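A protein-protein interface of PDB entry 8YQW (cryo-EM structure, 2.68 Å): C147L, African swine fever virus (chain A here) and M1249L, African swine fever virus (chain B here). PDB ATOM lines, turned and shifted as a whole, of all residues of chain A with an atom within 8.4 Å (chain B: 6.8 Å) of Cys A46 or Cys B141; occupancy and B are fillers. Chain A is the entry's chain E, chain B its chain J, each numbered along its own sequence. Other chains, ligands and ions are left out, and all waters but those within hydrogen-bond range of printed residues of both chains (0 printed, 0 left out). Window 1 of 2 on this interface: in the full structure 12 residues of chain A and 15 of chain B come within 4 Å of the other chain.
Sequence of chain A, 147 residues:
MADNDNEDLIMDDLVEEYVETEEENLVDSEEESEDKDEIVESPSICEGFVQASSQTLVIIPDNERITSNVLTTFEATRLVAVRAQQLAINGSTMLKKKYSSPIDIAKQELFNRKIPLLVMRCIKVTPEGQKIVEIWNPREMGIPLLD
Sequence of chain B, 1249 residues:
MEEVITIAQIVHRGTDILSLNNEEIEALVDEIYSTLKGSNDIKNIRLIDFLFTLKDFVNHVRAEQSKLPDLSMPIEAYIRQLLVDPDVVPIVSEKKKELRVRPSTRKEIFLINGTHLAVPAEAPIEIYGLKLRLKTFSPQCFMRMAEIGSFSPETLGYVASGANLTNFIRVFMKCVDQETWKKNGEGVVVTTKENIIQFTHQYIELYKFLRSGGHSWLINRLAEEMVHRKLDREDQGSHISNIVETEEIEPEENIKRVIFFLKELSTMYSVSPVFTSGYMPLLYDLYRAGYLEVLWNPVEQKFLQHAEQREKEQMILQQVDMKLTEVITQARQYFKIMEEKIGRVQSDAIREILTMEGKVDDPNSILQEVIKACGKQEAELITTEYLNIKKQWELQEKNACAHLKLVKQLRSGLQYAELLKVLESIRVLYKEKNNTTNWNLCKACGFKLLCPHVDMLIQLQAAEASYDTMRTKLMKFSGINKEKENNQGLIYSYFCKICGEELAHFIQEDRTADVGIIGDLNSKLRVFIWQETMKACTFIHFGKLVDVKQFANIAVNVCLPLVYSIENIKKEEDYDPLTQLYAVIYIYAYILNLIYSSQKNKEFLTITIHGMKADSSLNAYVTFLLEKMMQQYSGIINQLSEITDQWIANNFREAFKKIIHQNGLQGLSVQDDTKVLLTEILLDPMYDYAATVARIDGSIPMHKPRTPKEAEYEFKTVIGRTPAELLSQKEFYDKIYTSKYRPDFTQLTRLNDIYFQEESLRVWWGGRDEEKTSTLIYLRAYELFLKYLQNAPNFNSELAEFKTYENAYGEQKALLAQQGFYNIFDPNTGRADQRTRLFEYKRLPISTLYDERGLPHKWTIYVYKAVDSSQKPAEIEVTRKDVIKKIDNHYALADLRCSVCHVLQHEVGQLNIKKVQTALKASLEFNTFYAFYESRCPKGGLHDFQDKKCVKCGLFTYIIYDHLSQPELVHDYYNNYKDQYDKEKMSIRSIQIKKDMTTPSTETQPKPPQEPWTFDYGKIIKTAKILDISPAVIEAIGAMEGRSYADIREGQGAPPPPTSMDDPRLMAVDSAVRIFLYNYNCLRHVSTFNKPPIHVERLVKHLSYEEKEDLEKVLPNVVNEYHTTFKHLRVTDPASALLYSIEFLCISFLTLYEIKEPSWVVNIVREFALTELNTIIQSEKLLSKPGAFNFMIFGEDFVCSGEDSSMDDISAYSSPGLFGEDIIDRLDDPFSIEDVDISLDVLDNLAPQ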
ATOM      1  N   SER A  42      -3.872  17.033  11.318  1.00  0.00           N
ATOM      2  CA  SER A  42      -3.206  16.344  10.228  1.00  0.00           C
ATOM      3  C   SER A  42      -3.453  17.059   8.901  1.00  0.00           C
ATOM      4  O   SER A  42      -4.458  17.753   8.737  1.00  0.00           O
ATOM      5  CB  SER A  42      -3.700  14.902  10.151  1.00  0.00           C
ATOM      6  OG  SER A  42      -3.471  14.222  11.373  1.00  0.00           O
ATOM      7  N   PRO A  43      -2.533  16.918   7.942  1.00  0.00           N
ATOM      8  CA  PRO A  43      -2.726  17.567   6.640  1.00  0.00           C
ATOM      9  C   PRO A  43      -3.978  17.064   5.940  1.00  0.00           C
ATOM     10  O   PRO A  43      -4.322  15.882   6.001  1.00  0.00           O
ATOM     11  CB  PRO A  43      -1.458  17.188   5.862  1.00  0.00           C
ATOM     12  CG  PRO A  43      -0.936  15.972   6.550  1.00  0.00           C
ATOM     13  CD  PRO A  43      -1.273  16.158   7.996  1.00  0.00           C
ATOM     14  N   SER A  44      -4.657  17.983   5.263  1.00  0.00           N
ATOM     15  CA  SER A  44      -5.908  17.705   4.578  1.00  0.00           C
ATOM     16  C   SER A  44      -5.696  17.739   3.067  1.00  0.00           C
ATOM     17  O   SER A  44      -4.660  18.183   2.567  1.00  0.00           O
ATOM     18  CB  SER A  44      -6.985  18.704   5.008  1.00  0.00           C
ATOM     19  OG  SER A  44      -6.593  20.034   4.714  1.00  0.00           O
ATOM     20  N   ILE A  45      -6.704  17.258   2.337  1.00  0.00           N
ATOM     21  CA  ILE A  45      -6.639  17.258   0.880  1.00  0.00           C
ATOM     22  C   ILE A  45      -6.734  18.666   0.304  1.00  0.00           C
ATOM     23  O   ILE A  45      -6.293  18.893  -0.830  1.00  0.00           O
ATOM     24  CB  ILE A  45      -7.741  16.352   0.302  1.00  0.00           C
ATOM     25  CG1 ILE A  45      -7.794  15.032   1.073  1.00  0.00           C
ATOM     26  CG2 ILE A  45      -7.497  16.070  -1.173  1.00  0.00           C
ATOM     27  CD1 ILE A  45      -9.049  14.224   0.830  1.00  0.00           C
ATOM     28  N   CYS A  46      -7.284  19.623   1.056  1.00  0.00           N
ATOM     29  CA  CYS A  46      -7.386  20.989   0.552  1.00  0.00           C
ATOM     30  C   CYS A  46      -6.010  21.580   0.262  1.00  0.00           C
ATOM     31  O   CYS A  46      -5.854  22.376  -0.670  1.00  0.00           O
ATOM     32  CB  CYS A  46      -8.162  21.860   1.540  1.00  0.00           C
ATOM     33  SG  CYS A  46      -7.454  21.963   3.195  1.00  0.00           S
ATOM     34  N   GLU A  47      -5.005  21.208   1.048  1.00  0.00           N
ATOM     35  CA  GLU A  47      -3.627  21.472   0.666  1.00  0.00           C
ATOM     36  C   GLU A  47      -2.981  20.188   0.151  1.00  0.00           C
ATOM     37  O   GLU A  47      -3.604  19.125   0.095  1.00  0.00           O
ATOM     38  CB  GLU A  47      -2.821  22.055   1.830  1.00  0.00           C
ATOM     39  CG  GLU A  47      -2.570  21.109   2.991  1.00  0.00           C
ATOM     40  CD  GLU A  47      -3.479  21.381   4.172  1.00  0.00           C
ATOM     41  OE1 GLU A  47      -4.506  22.058   3.983  1.00  0.00           O
ATOM     42  OE2 GLU A  47      -3.160  20.924   5.290  1.00  0.00           O
ATOM     43  N   GLY A  48      -1.715  20.293  -0.231  1.00  0.00           N
ATOM     44  CA  GLY A  48      -1.020  19.182  -0.843  1.00  0.00           C
ATOM     45  C   GLY A  48      -1.190  19.067  -2.340  1.00  0.00           C
ATOM     46  O   GLY A  48      -0.701  18.095  -2.929  1.00  0.00           O
ATOM     47  N   PHE A  49      -1.872  20.018  -2.974  1.00  0.00           N
ATOM     48  CA  PHE A  49      -1.996  20.036  -4.424  1.00  0.00           C
ATOM     49  C   PHE A  49      -0.656  20.388  -5.048  1.00  0.00           C
ATOM     50  O   PHE A  49      -0.001  21.349  -4.632  1.00  0.00           O
ATOM     51  CB  PHE A  49      -3.055  21.047  -4.859  1.00  0.00           C
ATOM     52  CG  PHE A  49      -4.462  20.575  -4.663  1.00  0.00           C
ATOM     53  CD1 PHE A  49      -4.983  19.565  -5.448  1.00  0.00           C
ATOM     54  CD2 PHE A  49      -5.268  21.148  -3.697  1.00  0.00           C
ATOM     55  CE1 PHE A  49      -6.281  19.133  -5.271  1.00  0.00           C
ATOM     56  CE2 PHE A  49      -6.565  20.720  -3.515  1.00  0.00           C
ATOM     57  CZ  PHE A  49      -7.071  19.712  -4.302  1.00  0.00           C
ATOM     58  N   VAL A  50      -0.245  19.610  -6.045  1.00  0.00           N
ATOM     59  CA  VAL A  50       1.005  19.872  -6.747  1.00  0.00           C
ATOM     60  C   VAL A  50       0.688  20.588  -8.052  1.00  0.00           C
ATOM     61  O   VAL A  50       1.469  21.419  -8.526  1.00  0.00           O
ATOM     62  CB  VAL A  50       1.792  18.573  -6.999  1.00  0.00           C
ATOM     63  CG1 VAL A  50       3.144  18.880  -7.617  1.00  0.00           C
ATOM     64  CG2 VAL A  50       1.956  17.800  -5.702  1.00  0.00           C
ATOM     65  N   LYS B 135     -14.871  18.872   9.294  1.00  0.00           N
ATOM     66  CA  LYS B 135     -13.899  19.666   8.558  1.00  0.00           C
ATOM     67  C   LYS B 135     -14.591  20.721   7.708  1.00  0.00           C
ATOM     68  O   LYS B 135     -15.662  20.488   7.145  1.00  0.00           O
ATOM     69  CB  LYS B 135     -13.039  18.765   7.672  1.00  0.00           C
ATOM     70  CG  LYS B 135     -12.040  17.918   8.437  1.00  0.00           C
ATOM     71  CD  LYS B 135     -11.116  18.785   9.272  1.00  0.00           C
ATOM     72  CE  LYS B 135     -10.236  19.663   8.396  1.00  0.00           C
ATOM     73  NZ  LYS B 135      -9.236  18.864   7.640  1.00  0.00           N
ATOM     74  N   THR B 136     -13.970  21.893   7.624  1.00  0.00           N
ATOM     75  CA  THR B 136     -14.456  22.980   6.791  1.00  0.00           C
ATOM     76  C   THR B 136     -13.387  23.372   5.778  1.00  0.00           C
ATOM     77  O   THR B 136     -12.194  23.412   6.097  1.00  0.00           O
ATOM     78  CB  THR B 136     -14.863  24.192   7.637  1.00  0.00           C
ATOM     79  OG1 THR B 136     -15.387  25.219   6.786  1.00  0.00           O
ATOM     80  CG2 THR B 136     -13.680  24.735   8.431  1.00  0.00           C
ATOM     81  N   PHE B 137     -13.822  23.632   4.548  1.00  0.00           N
ATOM     82  CA  PHE B 137     -12.915  24.053   3.490  1.00  0.00           C
ATOM     83  C   PHE B 137     -13.450  25.306   2.812  1.00  0.00           C
ATOM     84  O   PHE B 137     -14.414  25.915   3.284  1.00  0.00           O
ATOM     85  CB  PHE B 137     -12.722  22.941   2.458  1.00  0.00           C
ATOM     86  CG  PHE B 137     -12.353  21.612   3.054  1.00  0.00           C
ATOM     87  CD1 PHE B 137     -11.149  21.443   3.714  1.00  0.00           C
ATOM     88  CD2 PHE B 137     -13.204  20.527   2.934  1.00  0.00           C
ATOM     89  CE1 PHE B 137     -10.807  20.218   4.256  1.00  0.00           C
ATOM     90  CE2 PHE B 137     -12.869  19.302   3.473  1.00  0.00           C
ATOM     91  CZ  PHE B 137     -11.670  19.146   4.135  1.00  0.00           C
ATOM     92  N   SER B 138     -12.829  25.696   1.711  1.00  0.00           N
ATOM     93  CA  SER B 138     -13.341  26.766   0.882  1.00  0.00           C
ATOM     94  C   SER B 138     -13.896  26.195  -0.417  1.00  0.00           C
ATOM     95  O   SER B 138     -13.459  25.131  -0.867  1.00  0.00           O
ATOM     96  CB  SER B 138     -12.248  27.789   0.556  1.00  0.00           C
ATOM     97  OG  SER B 138     -11.163  27.174  -0.114  1.00  0.00           O
ATOM     98  N   PRO B 139     -14.867  26.862  -1.042  1.00  0.00           N
ATOM     99  CA  PRO B 139     -15.311  26.416  -2.372  1.00  0.00           C
ATOM    100  C   PRO B 139     -14.212  26.488  -3.414  1.00  0.00           C
ATOM    101  O   PRO B 139     -14.328  25.842  -4.463  1.00  0.00           O
ATOM    102  CB  PRO B 139     -16.466  27.372  -2.699  1.00  0.00           C
ATOM    103  CG  PRO B 139     -16.920  27.886  -1.370  1.00  0.00           C
ATOM    104  CD  PRO B 139     -15.684  27.975  -0.532  1.00  0.00           C
ATOM    105  N   GLN B 140     -13.148  27.252  -3.156  1.00  0.00           N
ATOM    106  CA  GLN B 140     -12.013  27.282  -4.069  1.00  0.00           C
ATOM    107  C   GLN B 140     -11.325  25.925  -4.150  1.00  0.00           C
ATOM    108  O   GLN B 140     -10.820  25.552  -5.212  1.00  0.00           O
ATOM    109  CB  GLN B 140     -11.020  28.359  -3.634  1.00  0.00           C
ATOM    110  CG  GLN B 140     -11.544  29.779  -3.783  1.00  0.00           C
ATOM    111  CD  GLN B 140     -11.330  30.342  -5.175  1.00  0.00           C
ATOM    112  OE1 GLN B 140     -10.234  30.787  -5.516  1.00  0.00           O
ATOM    113  NE2 GLN B 140     -12.380  30.323  -5.988  1.00  0.00           N
ATOM    114  N   CYS B 141     -11.298  25.171  -3.047  1.00  0.00           N
ATOM    115  CA  CYS B 141     -10.729  23.827  -3.086  1.00  0.00           C
ATOM    116  C   CYS B 141     -11.539  22.904  -3.989  1.00  0.00           C
ATOM    117  O   CYS B 141     -10.970  22.140  -4.779  1.00  0.00           O
ATOM    118  CB  CYS B 141     -10.644  23.251  -1.674  1.00  0.00           C
ATOM    119  SG  CYS B 141     -10.146  21.517  -1.615  1.00  0.00           S
ATOM    120  N   PHE B 142     -12.868  22.958  -3.885  1.00  0.00           N
ATOM    121  CA  PHE B 142     -13.714  22.159  -4.765  1.00  0.00           C
ATOM    122  C   PHE B 142     -13.564  22.599  -6.214  1.00  0.00           C
ATOM    123  O   PHE B 142     -13.561  21.764  -7.127  1.00  0.00           O
ATOM    124  CB  PHE B 142     -15.172  22.254  -4.318  1.00  0.00           C
ATOM    125  CG  PHE B 142     -16.095  21.336  -5.060  1.00  0.00           C
ATOM    126  CD1 PHE B 142     -16.250  20.021  -4.663  1.00  0.00           C
ATOM    127  CD2 PHE B 142     -16.814  21.789  -6.152  1.00  0.00           C
ATOM    128  CE1 PHE B 142     -17.100  19.175  -5.342  1.00  0.00           C
ATOM    129  CE2 PHE B 142     -17.666  20.950  -6.833  1.00  0.00           C
ATOM    130  CZ  PHE B 142     -17.809  19.640  -6.428  1.00  0.00           C
ATOM    131  N   MET B 143     -13.441  23.909  -6.445  1.00  0.00           N
ATOM    132  CA  MET B 143     -13.203  24.403  -7.797  1.00  0.00           C
ATOM    133  C   MET B 143     -11.888  23.878  -8.353  1.00  0.00           C
ATOM    134  O   MET B 143     -11.815  23.487  -9.520  1.00  0.00           O
ATOM    135  CB  MET B 143     -13.217  25.930  -7.813  1.00  0.00           C
ATOM    136  CG  MET B 143     -14.594  26.536  -7.640  1.00  0.00           C
ATOM    137  SD  MET B 143     -15.701  26.064  -8.979  1.00  0.00           S
ATOM    138  CE  MET B 143     -16.714  24.853  -8.145  1.00  0.00           C
ATOM    139  N   ARG B 144     -10.838  23.863  -7.532  1.00  0.00           N
ATOM    140  CA  ARG B 144      -9.551  23.347  -7.981  1.00  0.00           C
ATOM    141  C   ARG B 144      -9.624  21.854  -8.277  1.00  0.00           C
ATOM    142  O   ARG B 144      -9.040  21.382  -9.261  1.00  0.00           O
ATOM    143  CB  ARG B 144      -8.481  23.643  -6.933  1.00  0.00           C
ATOM    144  CG  ARG B 144      -7.072  23.727  -7.485  1.00  0.00           C
ATOM    145  CD  ARG B 144      -6.094  24.157  -6.406  1.00  0.00           C
ATOM    146  NE  ARG B 144      -4.714  24.140  -6.872  1.00  0.00           N
ATOM    147  CZ  ARG B 144      -3.659  24.269  -6.080  1.00  0.00           C
ATOM    148  NH1 ARG B 144      -3.792  24.430  -4.773  1.00  0.00           N
ATOM    149  NH2 ARG B 144      -2.441  24.231  -6.609  1.00  0.00           N
ATOM    150  N   MET B 145     -10.329  21.091  -7.439  1.00  0.00           N
ATOM    151  CA  MET B 145     -10.455  19.658  -7.694  1.00  0.00           C
ATOM    152  C   MET B 145     -11.239  19.388  -8.972  1.00  0.00           C
ATOM    153  O   MET B 145     -10.895  18.479  -9.735  1.00  0.00           O
ATOM    154  CB  MET B 145     -11.115  18.952  -6.514  1.00  0.00           C
ATOM    155  CG  MET B 145     -10.346  19.026  -5.215  1.00  0.00           C
ATOM    156  SD  MET B 145     -10.840  17.692  -4.121  1.00  0.00           S
ATOM    157  CE  MET B 145     -12.613  17.832  -4.265  1.00  0.00           C
ATOM    158  N   ALA B 146     -12.305  20.153  -9.215  1.00  0.00           N
ATOM    159  CA  ALA B 146     -13.038  20.005 -10.468  1.00  0.00           C
ATOM    160  C   ALA B 146     -12.200  20.458 -11.657  1.00  0.00           C
ATOM    161  O   ALA B 146     -12.340  19.915 -12.759  1.00  0.00           O
ATOM    162  CB  ALA B 146     -14.350  20.784 -10.408  1.00  0.00           C
ATOM    163  N   GLU B 147     -11.337  21.454 -11.450  1.00  0.00           N
ATOM    164  CA  GLU B 147     -10.400  21.875 -12.483  1.00  0.00           C
ATOM    165  C   GLU B 147      -9.456  20.740 -12.852  1.00  0.00           C
ATOM    166  O   GLU B 147      -9.193  20.500 -14.036  1.00  0.00           O
ATOM    167  CB  GLU B 147      -9.603  23.097 -12.020  1.00  0.00           C
ATOM    168  CG  GLU B 147     -10.437  24.357 -11.859  1.00  0.00           C
ATOM    169  CD  GLU B 147      -9.627  25.527 -11.331  1.00  0.00           C
ATOM    170  OE1 GLU B 147      -8.471  25.309 -10.913  1.00  0.00           O
ATOM    171  OE2 GLU B 147     -10.148  26.662 -11.333  1.00  0.00           O
ATOM    172  N   VAL B 159     -15.189  16.742   0.059  1.00  0.00           N
ATOM    173  CA  VAL B 159     -14.772  18.142   0.075  1.00  0.00           C
ATOM    174  C   VAL B 159     -15.970  19.067  -0.109  1.00  0.00           C
ATOM    175  O   VAL B 159     -16.040  20.141   0.501  1.00  0.00           O
ATOM    176  CB  VAL B 159     -13.686  18.388  -0.986  1.00  0.00           C
ATOM    177  CG1 VAL B 159     -13.395  19.872  -1.125  1.00  0.00           C
ATOM    178  CG2 VAL B 159     -12.421  17.632  -0.621  1.00  0.00           C
ATOM    179  N   ALA B 163     -16.867  22.000   2.301  1.00  0.00           N
ATOM    180  CA  ALA B 163     -16.949  23.386   1.865  1.00  0.00           C
ATOM    181  C   ALA B 163     -18.377  23.915   1.849  1.00  0.00           C
ATOM    182  O   ALA B 163     -18.618  24.992   1.296  1.00  0.00           O
ATOM    183  CB  ALA B 163     -16.323  23.540   0.477  1.00  0.00           C
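The side-chain hydroxyl of Ser A44 lies within hydrogen-bond range of the side-chain carboxylate of Glu A47, 3.0 Å away. SG of Cys A46 sits at hydrogen-bond distance from OG of Ser A44, 2.6 Å away. The side-chain sulfur of Cys A46 is in hydrogen-bond range of the side-chain carboxylate of Glu A47 (3.1 Å).
Of the 15 printed residues of chain B, 5 touch a printed residue of chain A. Of the 9 printed residues of chain A, 3 touch a printed residue of chain B. Hydrophobic or aromatic side chains of chain A that line the printed part of chain B: Phe A49. Among the printed residues, no Asp or Glu carboxylate lies within 4 Å of a Lys or Arg side-chain nitrogen of the other chain.
Cys A46 touches just these residues of chain B: Phe B137 (3.7 Å) and Cys B141 (3.5 Å). Cys B141 touches one residue of chain A. Of the printed residues of chain B, Ser A44 touches Lys B135. Of the printed residues of chain A, Met B145 touches Phe A49. Printed residues of chain A within 4 Å of Lys B135: Ser A44. Of the printed residues of chain B, Phe A49 touches Arg B144 (3.5 Å) and Met B145 (3.5 Å). Of the printed residues of chain A, Phe B137 touches Cys A46. The nearest residue of chain A that does not touch Cys B141 is Phe A49 (4.1 Å). The nearest printed residue of chain A that does not touch Phe B137 is Ser A44 (4.2 Å).
NZ of Lys B135 touches CB of Ser A44, 3.5 Å away. CD1 of Phe B137 touches CB of Cys A46 (3.7 Å). CA of Cys A46 touches SG of Cys B141 (3.5 Å). NH1 of Arg B144 touches CB of Phe A49, at 3.5 Å. Phe A49 touches Met B145.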
